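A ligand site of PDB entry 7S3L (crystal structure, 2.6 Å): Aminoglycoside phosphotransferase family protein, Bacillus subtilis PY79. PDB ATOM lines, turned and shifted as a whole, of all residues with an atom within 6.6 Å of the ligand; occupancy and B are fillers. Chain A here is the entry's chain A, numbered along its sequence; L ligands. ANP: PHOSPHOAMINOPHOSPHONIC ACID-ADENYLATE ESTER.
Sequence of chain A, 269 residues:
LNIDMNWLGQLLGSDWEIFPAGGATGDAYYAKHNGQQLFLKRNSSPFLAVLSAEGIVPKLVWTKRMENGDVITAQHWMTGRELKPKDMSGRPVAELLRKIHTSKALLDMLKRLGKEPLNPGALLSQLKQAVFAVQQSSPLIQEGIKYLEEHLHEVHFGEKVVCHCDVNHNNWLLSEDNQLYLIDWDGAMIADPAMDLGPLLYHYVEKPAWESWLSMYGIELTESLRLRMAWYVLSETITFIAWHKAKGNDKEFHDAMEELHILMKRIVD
N of His 76 is in hydrogen-bond range of O of Lys 59 (3.1 Å). N of Trp 77 sits close to O of Gln 37 (3.4 Å). The backbone carbonyl oxygen of Phe 39 is in hydrogen-bond range of the backbone NH of Gln 75 (2.8 Å). The side-chain amide nitrogen (NE2) of Gln 75 is in hydrogen-bond range of the backbone carbonyl oxygen (O) of Pro 58 (2.8 Å). The backbone carbonyl oxygen of Thr 79 is in hydrogen-bond range of the backbone NH of Glu 176, at 2.9 Å.
Merely in contact with the ligand: Phe 39 (3.4 Å), Pro 58 (3.4 Å), Gln 75 (3.6 Å), Thr 79 (3.7 Å), Leu 173 (3.9 Å) and Ile 183 (3.8 Å). Hydrophobic or aromatic side chains that line the ligand: Phe 39, Pro 58, Trp 77, Met 78, Leu 173 and Ile 183. Ten residues have an atom within 4 Å of the ligand: Phe 39, Pro 58, Gln 75, His 76, Trp 77, Met 78, Thr 79, Gly 80, Leu 173 and Ile 183. Along chain A the residues within 4 Å of the ligand span positions 39 to 183. The nearest printed residue that does not touch the ligand is Arg 81 (4.7 Å).
The backbone NH of Gly 80 sits at hydrogen-bond distance from an oxygen (O1A) of the ligand, 3.0 Å away. O of Gly 80 lies close to O1A of the ligand (2.9 Å). N7 of the ligand sits at hydrogen-bond distance from N of Met 78. O of His 76 is in hydrogen-bond range of N6 of the ligand (3.1 Å). NE1 of Trp 77 lies within hydrogen-bond range of O2A of the ligand (3.2 Å).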
ATOM      1  N   ALA A  21     -21.035  12.082 -23.922  1.00  0.00           N
ATOM      2  CA  ALA A  21     -19.636  12.372 -23.642  1.00  0.00           C
ATOM      3  C   ALA A  21     -18.782  11.142 -23.954  1.00  0.00           C
ATOM      4  O   ALA A  21     -17.560  11.187 -23.900  1.00  0.00           O
ATOM      5  CB  ALA A  21     -19.465  12.812 -22.204  1.00  0.00           C
ATOM      6  N   THR A  25     -17.851   7.213 -20.224  1.00  0.00           N
ATOM      7  CA  THR A  25     -18.312   5.812 -20.168  1.00  0.00           C
ATOM      8  C   THR A  25     -19.747   5.742 -19.644  1.00  0.00           C
ATOM      9  O   THR A  25     -20.213   6.691 -19.018  1.00  0.00           O
ATOM     10  CB  THR A  25     -17.441   4.929 -19.228  1.00  0.00           C
ATOM     11  OG1 THR A  25     -17.892   5.118 -17.868  1.00  0.00           O
ATOM     12  CG2 THR A  25     -15.946   5.261 -19.332  1.00  0.00           C
ATOM     13  N   ALA A  28     -23.142   8.802 -20.391  1.00  0.00           N
ATOM     14  CA  ALA A  28     -22.598  10.106 -20.042  1.00  0.00           C
ATOM     15  C   ALA A  28     -22.916  11.132 -21.129  1.00  0.00           C
ATOM     16  O   ALA A  28     -22.507  10.964 -22.283  1.00  0.00           O
ATOM     17  CB  ALA A  28     -21.084  10.014 -19.813  1.00  0.00           C
ATOM     18  N   LYS A  32     -24.597  22.183 -21.500  1.00  0.00           N
ATOM     19  CA  LYS A  32     -23.987  23.515 -21.486  1.00  0.00           C
ATOM     20  C   LYS A  32     -25.034  24.614 -21.628  1.00  0.00           C
ATOM     21  O   LYS A  32     -25.878  24.558 -22.537  1.00  0.00           O
ATOM     22  CB  LYS A  32     -22.943  23.641 -22.607  1.00  0.00           C
ATOM     23  CG  LYS A  32     -21.629  22.975 -22.292  1.00  0.00           C
ATOM     24  CD  LYS A  32     -20.778  22.704 -23.532  1.00  0.00           C
ATOM     25  CE  LYS A  32     -19.597  21.817 -23.137  1.00  0.00           C
ATOM     26  NZ  LYS A  32     -18.888  21.158 -24.288  1.00  0.00           N
ATOM     27  N   GLN A  37     -21.536  24.026 -16.948  1.00  0.00           N
ATOM     28  CA  GLN A  37     -21.516  22.684 -17.513  1.00  0.00           C
ATOM     29  C   GLN A  37     -21.907  21.679 -16.446  1.00  0.00           C
ATOM     30  O   GLN A  37     -21.479  21.788 -15.290  1.00  0.00           O
ATOM     31  CB  GLN A  37     -20.148  22.322 -18.084  1.00  0.00           C
ATOM     32  CG  GLN A  37     -19.729  23.092 -19.302  1.00  0.00           C
ATOM     33  CD  GLN A  37     -18.369  22.616 -19.797  1.00  0.00           C
ATOM     34  OE1 GLN A  37     -18.244  21.507 -20.338  1.00  0.00           O
ATOM     35  NE2 GLN A  37     -17.337  23.432 -19.587  1.00  0.00           N
ATOM     36  N   LEU A  38     -22.701  20.701 -16.829  1.00  0.00           N
ATOM     37  CA  LEU A  38     -23.077  19.613 -15.954  1.00  0.00           C
ATOM     38  C   LEU A  38     -22.682  18.291 -16.585  1.00  0.00           C
ATOM     39  O   LEU A  38     -22.580  18.162 -17.809  1.00  0.00           O
ATOM     40  CB  LEU A  38     -24.568  19.635 -15.660  1.00  0.00           C
ATOM     41  CG  LEU A  38     -25.077  20.965 -15.092  1.00  0.00           C
ATOM     42  CD1 LEU A  38     -26.573  20.905 -14.906  1.00  0.00           C
ATOM     43  CD2 LEU A  38     -24.377  21.305 -13.775  1.00  0.00           C
ATOM     44  N   PHE A  39     -22.421  17.312 -15.741  1.00  0.00           N
ATOM     45  CA  PHE A  39     -22.205  15.948 -16.146  1.00  0.00           C
ATOM     46  C   PHE A  39     -23.474  15.196 -15.778  1.00  0.00           C
ATOM     47  O   PHE A  39     -23.843  15.162 -14.601  1.00  0.00           O
ATOM     48  CB  PHE A  39     -20.969  15.390 -15.440  1.00  0.00           C
ATOM     49  CG  PHE A  39     -20.543  14.012 -15.885  1.00  0.00           C
ATOM     50  CD1 PHE A  39     -21.132  12.884 -15.341  1.00  0.00           C
ATOM     51  CD2 PHE A  39     -19.522  13.851 -16.802  1.00  0.00           C
ATOM     52  CE1 PHE A  39     -20.743  11.622 -15.726  1.00  0.00           C
ATOM     53  CE2 PHE A  39     -19.119  12.587 -17.191  1.00  0.00           C
ATOM     54  CZ  PHE A  39     -19.738  11.472 -16.656  1.00  0.00           C
ATOM     55  N   VAL A  57     -16.127  11.819  -5.919  1.00  0.00           N
ATOM     56  CA  VAL A  57     -16.443  12.221  -7.291  1.00  0.00           C
ATOM     57  C   VAL A  57     -16.964  13.648  -7.238  1.00  0.00           C
ATOM     58  O   VAL A  57     -17.314  14.163  -6.154  1.00  0.00           O
ATOM     59  CB  VAL A  57     -17.454  11.261  -7.962  1.00  0.00           C
ATOM     60  CG1 VAL A  57     -16.921   9.854  -8.038  1.00  0.00           C
ATOM     61  CG2 VAL A  57     -18.797  11.275  -7.230  1.00  0.00           C
ATOM     62  N   PRO A  58     -16.999  14.345  -8.378  1.00  0.00           N
ATOM     63  CA  PRO A  58     -17.540  15.714  -8.384  1.00  0.00           C
ATOM     64  C   PRO A  58     -18.971  15.728  -7.865  1.00  0.00           C
ATOM     65  O   PRO A  58     -19.778  14.847  -8.175  1.00  0.00           O
ATOM     66  CB  PRO A  58     -17.450  16.129  -9.850  1.00  0.00           C
ATOM     67  CG  PRO A  58     -16.326  15.257 -10.419  1.00  0.00           C
ATOM     68  CD  PRO A  58     -16.507  13.955  -9.715  1.00  0.00           C
ATOM     69  N   LYS A  59     -19.289  16.737  -7.058  1.00  0.00           N
ATOM     70  CA  LYS A  59     -20.471  16.649  -6.210  1.00  0.00           C
ATOM     71  C   LYS A  59     -21.755  16.821  -7.012  1.00  0.00           C
ATOM     72  O   LYS A  59     -21.806  17.549  -8.004  1.00  0.00           O
ATOM     73  CB  LYS A  59     -20.395  17.667  -5.085  1.00  0.00           C
ATOM     74  CG  LYS A  59     -20.685  19.052  -5.482  1.00  0.00           C
ATOM     75  CD  LYS A  59     -20.879  19.923  -4.251  1.00  0.00           C
ATOM     76  CE  LYS A  59     -21.584  21.258  -4.570  1.00  0.00           C
ATOM     77  NZ  LYS A  59     -21.565  22.158  -3.387  1.00  0.00           N
ATOM     78  N   GLN A  75     -24.235  16.361 -12.084  1.00  0.00           N
ATOM     79  CA  GLN A  75     -23.044  16.592 -11.281  1.00  0.00           C
ATOM     80  C   GLN A  75     -22.292  17.813 -11.809  1.00  0.00           C
ATOM     81  O   GLN A  75     -22.371  18.126 -12.991  1.00  0.00           O
ATOM     82  CB  GLN A  75     -22.094  15.401 -11.297  1.00  0.00           C
ATOM     83  CG  GLN A  75     -22.467  14.262 -10.366  1.00  0.00           C
ATOM     84  CD  GLN A  75     -21.649  13.006 -10.656  1.00  0.00           C
ATOM     85  OE1 GLN A  75     -22.135  12.071 -11.278  1.00  0.00           O
ATOM     86  NE2 GLN A  75     -20.404  12.995 -10.199  1.00  0.00           N
ATOM     87  N   HIS A  76     -21.566  18.486 -10.932  1.00  0.00           N
ATOM     88  CA  HIS A  76     -20.615  19.479 -11.389  1.00  0.00           C
ATOM     89  C   HIS A  76     -19.729  18.883 -12.469  1.00  0.00           C
ATOM     90  O   HIS A  76     -19.227  17.761 -12.338  1.00  0.00           O
ATOM     91  CB  HIS A  76     -19.774  19.979 -10.216  1.00  0.00           C
ATOM     92  CG  HIS A  76     -18.668  20.904 -10.617  1.00  0.00           C
ATOM     93  ND1 HIS A  76     -18.903  22.112 -11.255  1.00  0.00           N
ATOM     94  CD2 HIS A  76     -17.328  20.801 -10.483  1.00  0.00           C
ATOM     95  CE1 HIS A  76     -17.755  22.704 -11.495  1.00  0.00           C
ATOM     96  NE2 HIS A  76     -16.775  21.937 -11.032  1.00  0.00           N
ATOM     97  N   TRP A  77     -19.577  19.604 -13.570  1.00  0.00           N
ATOM     98  CA  TRP A  77     -18.676  19.174 -14.627  1.00  0.00           C
ATOM     99  C   TRP A  77     -17.294  19.692 -14.276  1.00  0.00           C
ATOM    100  O   TRP A  77     -17.055  20.898 -14.274  1.00  0.00           O
ATOM    101  CB  TRP A  77     -19.116  19.669 -15.996  1.00  0.00           C
ATOM    102  CG  TRP A  77     -18.127  19.301 -17.060  1.00  0.00           C
ATOM    103  CD1 TRP A  77     -16.931  19.905 -17.318  1.00  0.00           C
ATOM    104  CD2 TRP A  77     -18.247  18.229 -18.002  1.00  0.00           C
ATOM    105  NE1 TRP A  77     -16.297  19.283 -18.364  1.00  0.00           N
ATOM    106  CE2 TRP A  77     -17.081  18.247 -18.802  1.00  0.00           C
ATOM    107  CE3 TRP A  77     -19.216  17.260 -18.251  1.00  0.00           C
ATOM    108  CZ2 TRP A  77     -16.871  17.329 -19.813  1.00  0.00           C
ATOM    109  CZ3 TRP A  77     -18.999  16.347 -19.266  1.00  0.00           C
ATOM    110  CH2 TRP A  77     -17.838  16.392 -20.043  1.00  0.00           C
ATOM    111  N   MET A  78     -16.377  18.781 -13.980  1.00  0.00           N
ATOM    112  CA  MET A  78     -15.057  19.173 -13.521  1.00  0.00           C
ATOM    113  C   MET A  78     -14.187  19.632 -14.699  1.00  0.00           C
ATOM    114  O   MET A  78     -14.239  19.073 -15.790  1.00  0.00           O
ATOM    115  CB  MET A  78     -14.398  18.011 -12.771  1.00  0.00           C
ATOM    116  CG  MET A  78     -13.445  17.112 -13.586  1.00  0.00           C
ATOM    117  SD  MET A  78     -11.638  17.150 -12.807  1.00  0.00           S
ATOM    118  CE  MET A  78     -12.333  17.811 -11.198  1.00  0.00           C
ATOM    119  N   THR A  79     -13.403  20.670 -14.442  1.00  0.00           N
ATOM    120  CA  THR A  79     -12.421  21.169 -15.387  1.00  0.00           C
ATOM    121  C   THR A  79     -11.030  20.781 -14.901  1.00  0.00           C
ATOM    122  O   THR A  79     -10.594  21.201 -13.830  1.00  0.00           O
ATOM    123  CB  THR A  79     -12.521  22.695 -15.526  1.00  0.00           C
ATOM    124  OG1 THR A  79     -13.844  23.051 -15.937  1.00  0.00           O
ATOM    125  CG2 THR A  79     -11.501  23.199 -16.540  1.00  0.00           C
ATOM    126  N   GLY A  80     -10.343  19.976 -15.697  1.00  0.00           N
ATOM    127  CA  GLY A  80      -8.985  19.592 -15.375  1.00  0.00           C
ATOM    128  C   GLY A  80      -8.484  18.525 -16.319  1.00  0.00           C
ATOM    129  O   GLY A  80      -8.790  18.556 -17.515  1.00  0.00           O
ATOM    130  N   ARG A  81      -7.744  17.564 -15.782  1.00  0.00           N
ATOM    131  CA  ARG A  81      -7.057  16.582 -16.589  1.00  0.00           C
ATOM    132  C   ARG A  81      -7.037  15.260 -15.853  1.00  0.00           C
ATOM    133  O   ARG A  81      -7.139  15.200 -14.634  1.00  0.00           O
ATOM    134  CB  ARG A  81      -5.635  17.025 -16.882  1.00  0.00           C
ATOM    135  CG  ARG A  81      -4.788  17.076 -15.633  1.00  0.00           C
ATOM    136  CD  ARG A  81      -3.304  17.156 -15.926  1.00  0.00           C
ATOM    137  NE  ARG A  81      -2.530  17.339 -14.705  1.00  0.00           N
ATOM    138  CZ  ARG A  81      -1.788  16.388 -14.129  1.00  0.00           C
ATOM    139  NH1 ARG A  81      -1.700  15.179 -14.670  1.00  0.00           N
ATOM    140  NH2 ARG A  81      -1.133  16.659 -13.016  1.00  0.00           N
ATOM    141  N   GLU A  82      -6.888  14.179 -16.616  1.00  0.00           N
ATOM    142  CA  GLU A  82      -6.561  12.915 -15.989  1.00  0.00           C
ATOM    143  C   GLU A  82      -5.163  12.979 -15.370  1.00  0.00           C
ATOM    144  O   GLU A  82      -4.356  13.865 -15.672  1.00  0.00           O
ATOM    145  CB  GLU A  82      -6.638  11.774 -16.991  1.00  0.00           C
ATOM    146  CG  GLU A  82      -7.954  11.691 -17.725  1.00  0.00           C
ATOM    147  CD  GLU A  82      -7.956  10.554 -18.760  1.00  0.00           C
ATOM    148  OE1 GLU A  82      -6.866  10.018 -19.065  1.00  0.00           O
ATOM    149  OE2 GLU A  82      -9.057  10.211 -19.256  1.00  0.00           O
ATOM    150  N   LEU A 173      -9.096  11.975 -11.655  1.00  0.00           N
ATOM    151  CA  LEU A 173      -9.261  13.318 -12.192  1.00  0.00           C
ATOM    152  C   LEU A 173      -8.660  14.351 -11.261  1.00  0.00           C
ATOM    153  O   LEU A 173      -8.703  14.196 -10.039  1.00  0.00           O
ATOM    154  CB  LEU A 173     -10.734  13.635 -12.420  1.00  0.00           C
ATOM    155  CG  LEU A 173     -11.494  12.704 -13.353  1.00  0.00           C
ATOM    156  CD1 LEU A 173     -12.950  13.150 -13.485  1.00  0.00           C
ATOM    157  CD2 LEU A 173     -10.804  12.644 -14.711  1.00  0.00           C
ATOM    158  N   GLU A 176      -8.723  22.060 -11.732  1.00  0.00           N
ATOM    159  CA  GLU A 176      -8.057  23.341 -11.552  1.00  0.00           C
ATOM    160  C   GLU A 176      -8.250  23.886 -10.152  1.00  0.00           C
ATOM    161  O   GLU A 176      -7.446  24.723  -9.719  1.00  0.00           O
ATOM    162  CB  GLU A 176      -8.579  24.336 -12.581  1.00  0.00           C
ATOM    163  CG  GLU A 176      -8.405  23.826 -13.992  1.00  0.00           C
ATOM    164  CD  GLU A 176      -8.896  24.805 -15.034  1.00  0.00           C
ATOM    165  OE1 GLU A 176      -9.731  25.680 -14.692  1.00  0.00           O
ATOM    166  OE2 GLU A 176      -8.442  24.701 -16.196  1.00  0.00           O
ATOM    167  N   ILE A 183     -13.142   8.043 -10.421  1.00  0.00           N
ATOM    168  CA  ILE A 183     -14.436   7.866 -11.052  1.00  0.00           C
ATOM    169  C   ILE A 183     -14.558   6.455 -11.615  1.00  0.00           C
ATOM    170  O   ILE A 183     -13.632   5.643 -11.524  1.00  0.00           O
ATOM    171  CB  ILE A 183     -14.701   8.893 -12.165  1.00  0.00           C
ATOM    172  CG1 ILE A 183     -13.640   8.714 -13.266  1.00  0.00           C
ATOM    173  CG2 ILE A 183     -14.763  10.297 -11.571  1.00  0.00           C
ATOM    174  CD1 ILE A 183     -13.837   9.604 -14.483  1.00  0.00           C
ATOM    175  N   ASP A 184     -15.715   6.198 -12.235  1.00  0.00           N
ATOM    176  CA  ASP A 184     -16.131   4.919 -12.800  1.00  0.00           C
ATOM    177  C   ASP A 184     -16.264   3.844 -11.737  1.00  0.00           C
ATOM    178  O   ASP A 184     -15.312   3.117 -11.477  1.00  0.00           O
ATOM    179  CB  ASP A 184     -15.168   4.458 -13.883  1.00  0.00           C
ATOM    180  CG  ASP A 184     -15.899   4.051 -15.128  1.00  0.00           C
ATOM    181  OD1 ASP A 184     -16.338   2.870 -15.200  1.00  0.00           O
ATOM    182  OD2 ASP A 184     -16.104   4.941 -15.992  1.00  0.00           O
HETATM  183  PG  ANP L   1     -11.239  20.490 -23.177  1.00  0.00           P
HETATM  184  O1G ANP L   1     -11.111  21.959 -23.444  1.00  0.00           O
HETATM  185  O2G ANP L   1     -12.749  20.155 -22.829  1.00  0.00           O
HETATM  186  O3G ANP L   1     -10.794  19.665 -24.463  1.00  0.00           O
HETATM  187  PB  ANP L   1     -10.340  18.459 -21.411  1.00  0.00           P
HETATM  188  O1B ANP L   1     -10.377  17.572 -22.651  1.00  0.00           O
HETATM  189  O2B ANP L   1      -9.125  18.086 -20.512  1.00  0.00           O
HETATM  190  N3B ANP L   1     -10.208  20.080 -21.872  1.00  0.00           N
HETATM  191  PA  ANP L   1     -12.231  18.989 -19.349  1.00  0.00           P
HETATM  192  O1A ANP L   1     -11.176  19.708 -18.604  1.00  0.00           O
HETATM  193  O2A ANP L   1     -13.436  19.815 -19.811  1.00  0.00           O
HETATM  194  O3A ANP L   1     -11.695  18.202 -20.644  1.00  0.00           O
HETATM  195  O5' ANP L   1     -12.659  17.769 -18.446  1.00  0.00           O
HETATM  196  C5' ANP L   1     -13.561  16.793 -19.004  1.00  0.00           C
HETATM  197  C4' ANP L   1     -13.109  15.401 -18.670  1.00  0.00           C
HETATM  198  O4' ANP L   1     -13.465  15.095 -17.305  1.00  0.00           O
HETATM  199  C3' ANP L   1     -13.798  14.313 -19.495  1.00  0.00           C
HETATM  200  O3' ANP L   1     -12.992  13.144 -19.516  1.00  0.00           O
HETATM  201  C2' ANP L   1     -15.088  14.117 -18.706  1.00  0.00           C
HETATM  202  O2' ANP L   1     -15.706  12.850 -18.950  1.00  0.00           O
HETATM  203  C1' ANP L   1     -14.544  14.182 -17.278  1.00  0.00           C
HETATM  204  N9  ANP L   1     -15.503  14.603 -16.281  1.00  0.00           N
HETATM  205  C8  ANP L   1     -15.863  15.880 -15.944  1.00  0.00           C
HETATM  206  N7  ANP L   1     -16.745  15.972 -14.976  1.00  0.00           N
HETATM  207  C5  ANP L   1     -16.989  14.627 -14.655  1.00  0.00           C
HETATM  208  C6  ANP L   1     -17.848  14.034 -13.713  1.00  0.00           C
HETATM  209  N6  ANP L   1     -18.640  14.715 -12.878  1.00  0.00           N
HETATM  210  N1  ANP L   1     -17.855  12.680 -13.655  1.00  0.00           N
HETATM  211  C2  ANP L   1     -17.064  11.986 -14.485  1.00  0.00           C
HETATM  212  N3  ANP L   1     -16.221  12.448 -15.408  1.00  0.00           N
HETATM  213  C4  ANP L   1     -16.239  13.798 -15.446  1.00  0.00           C
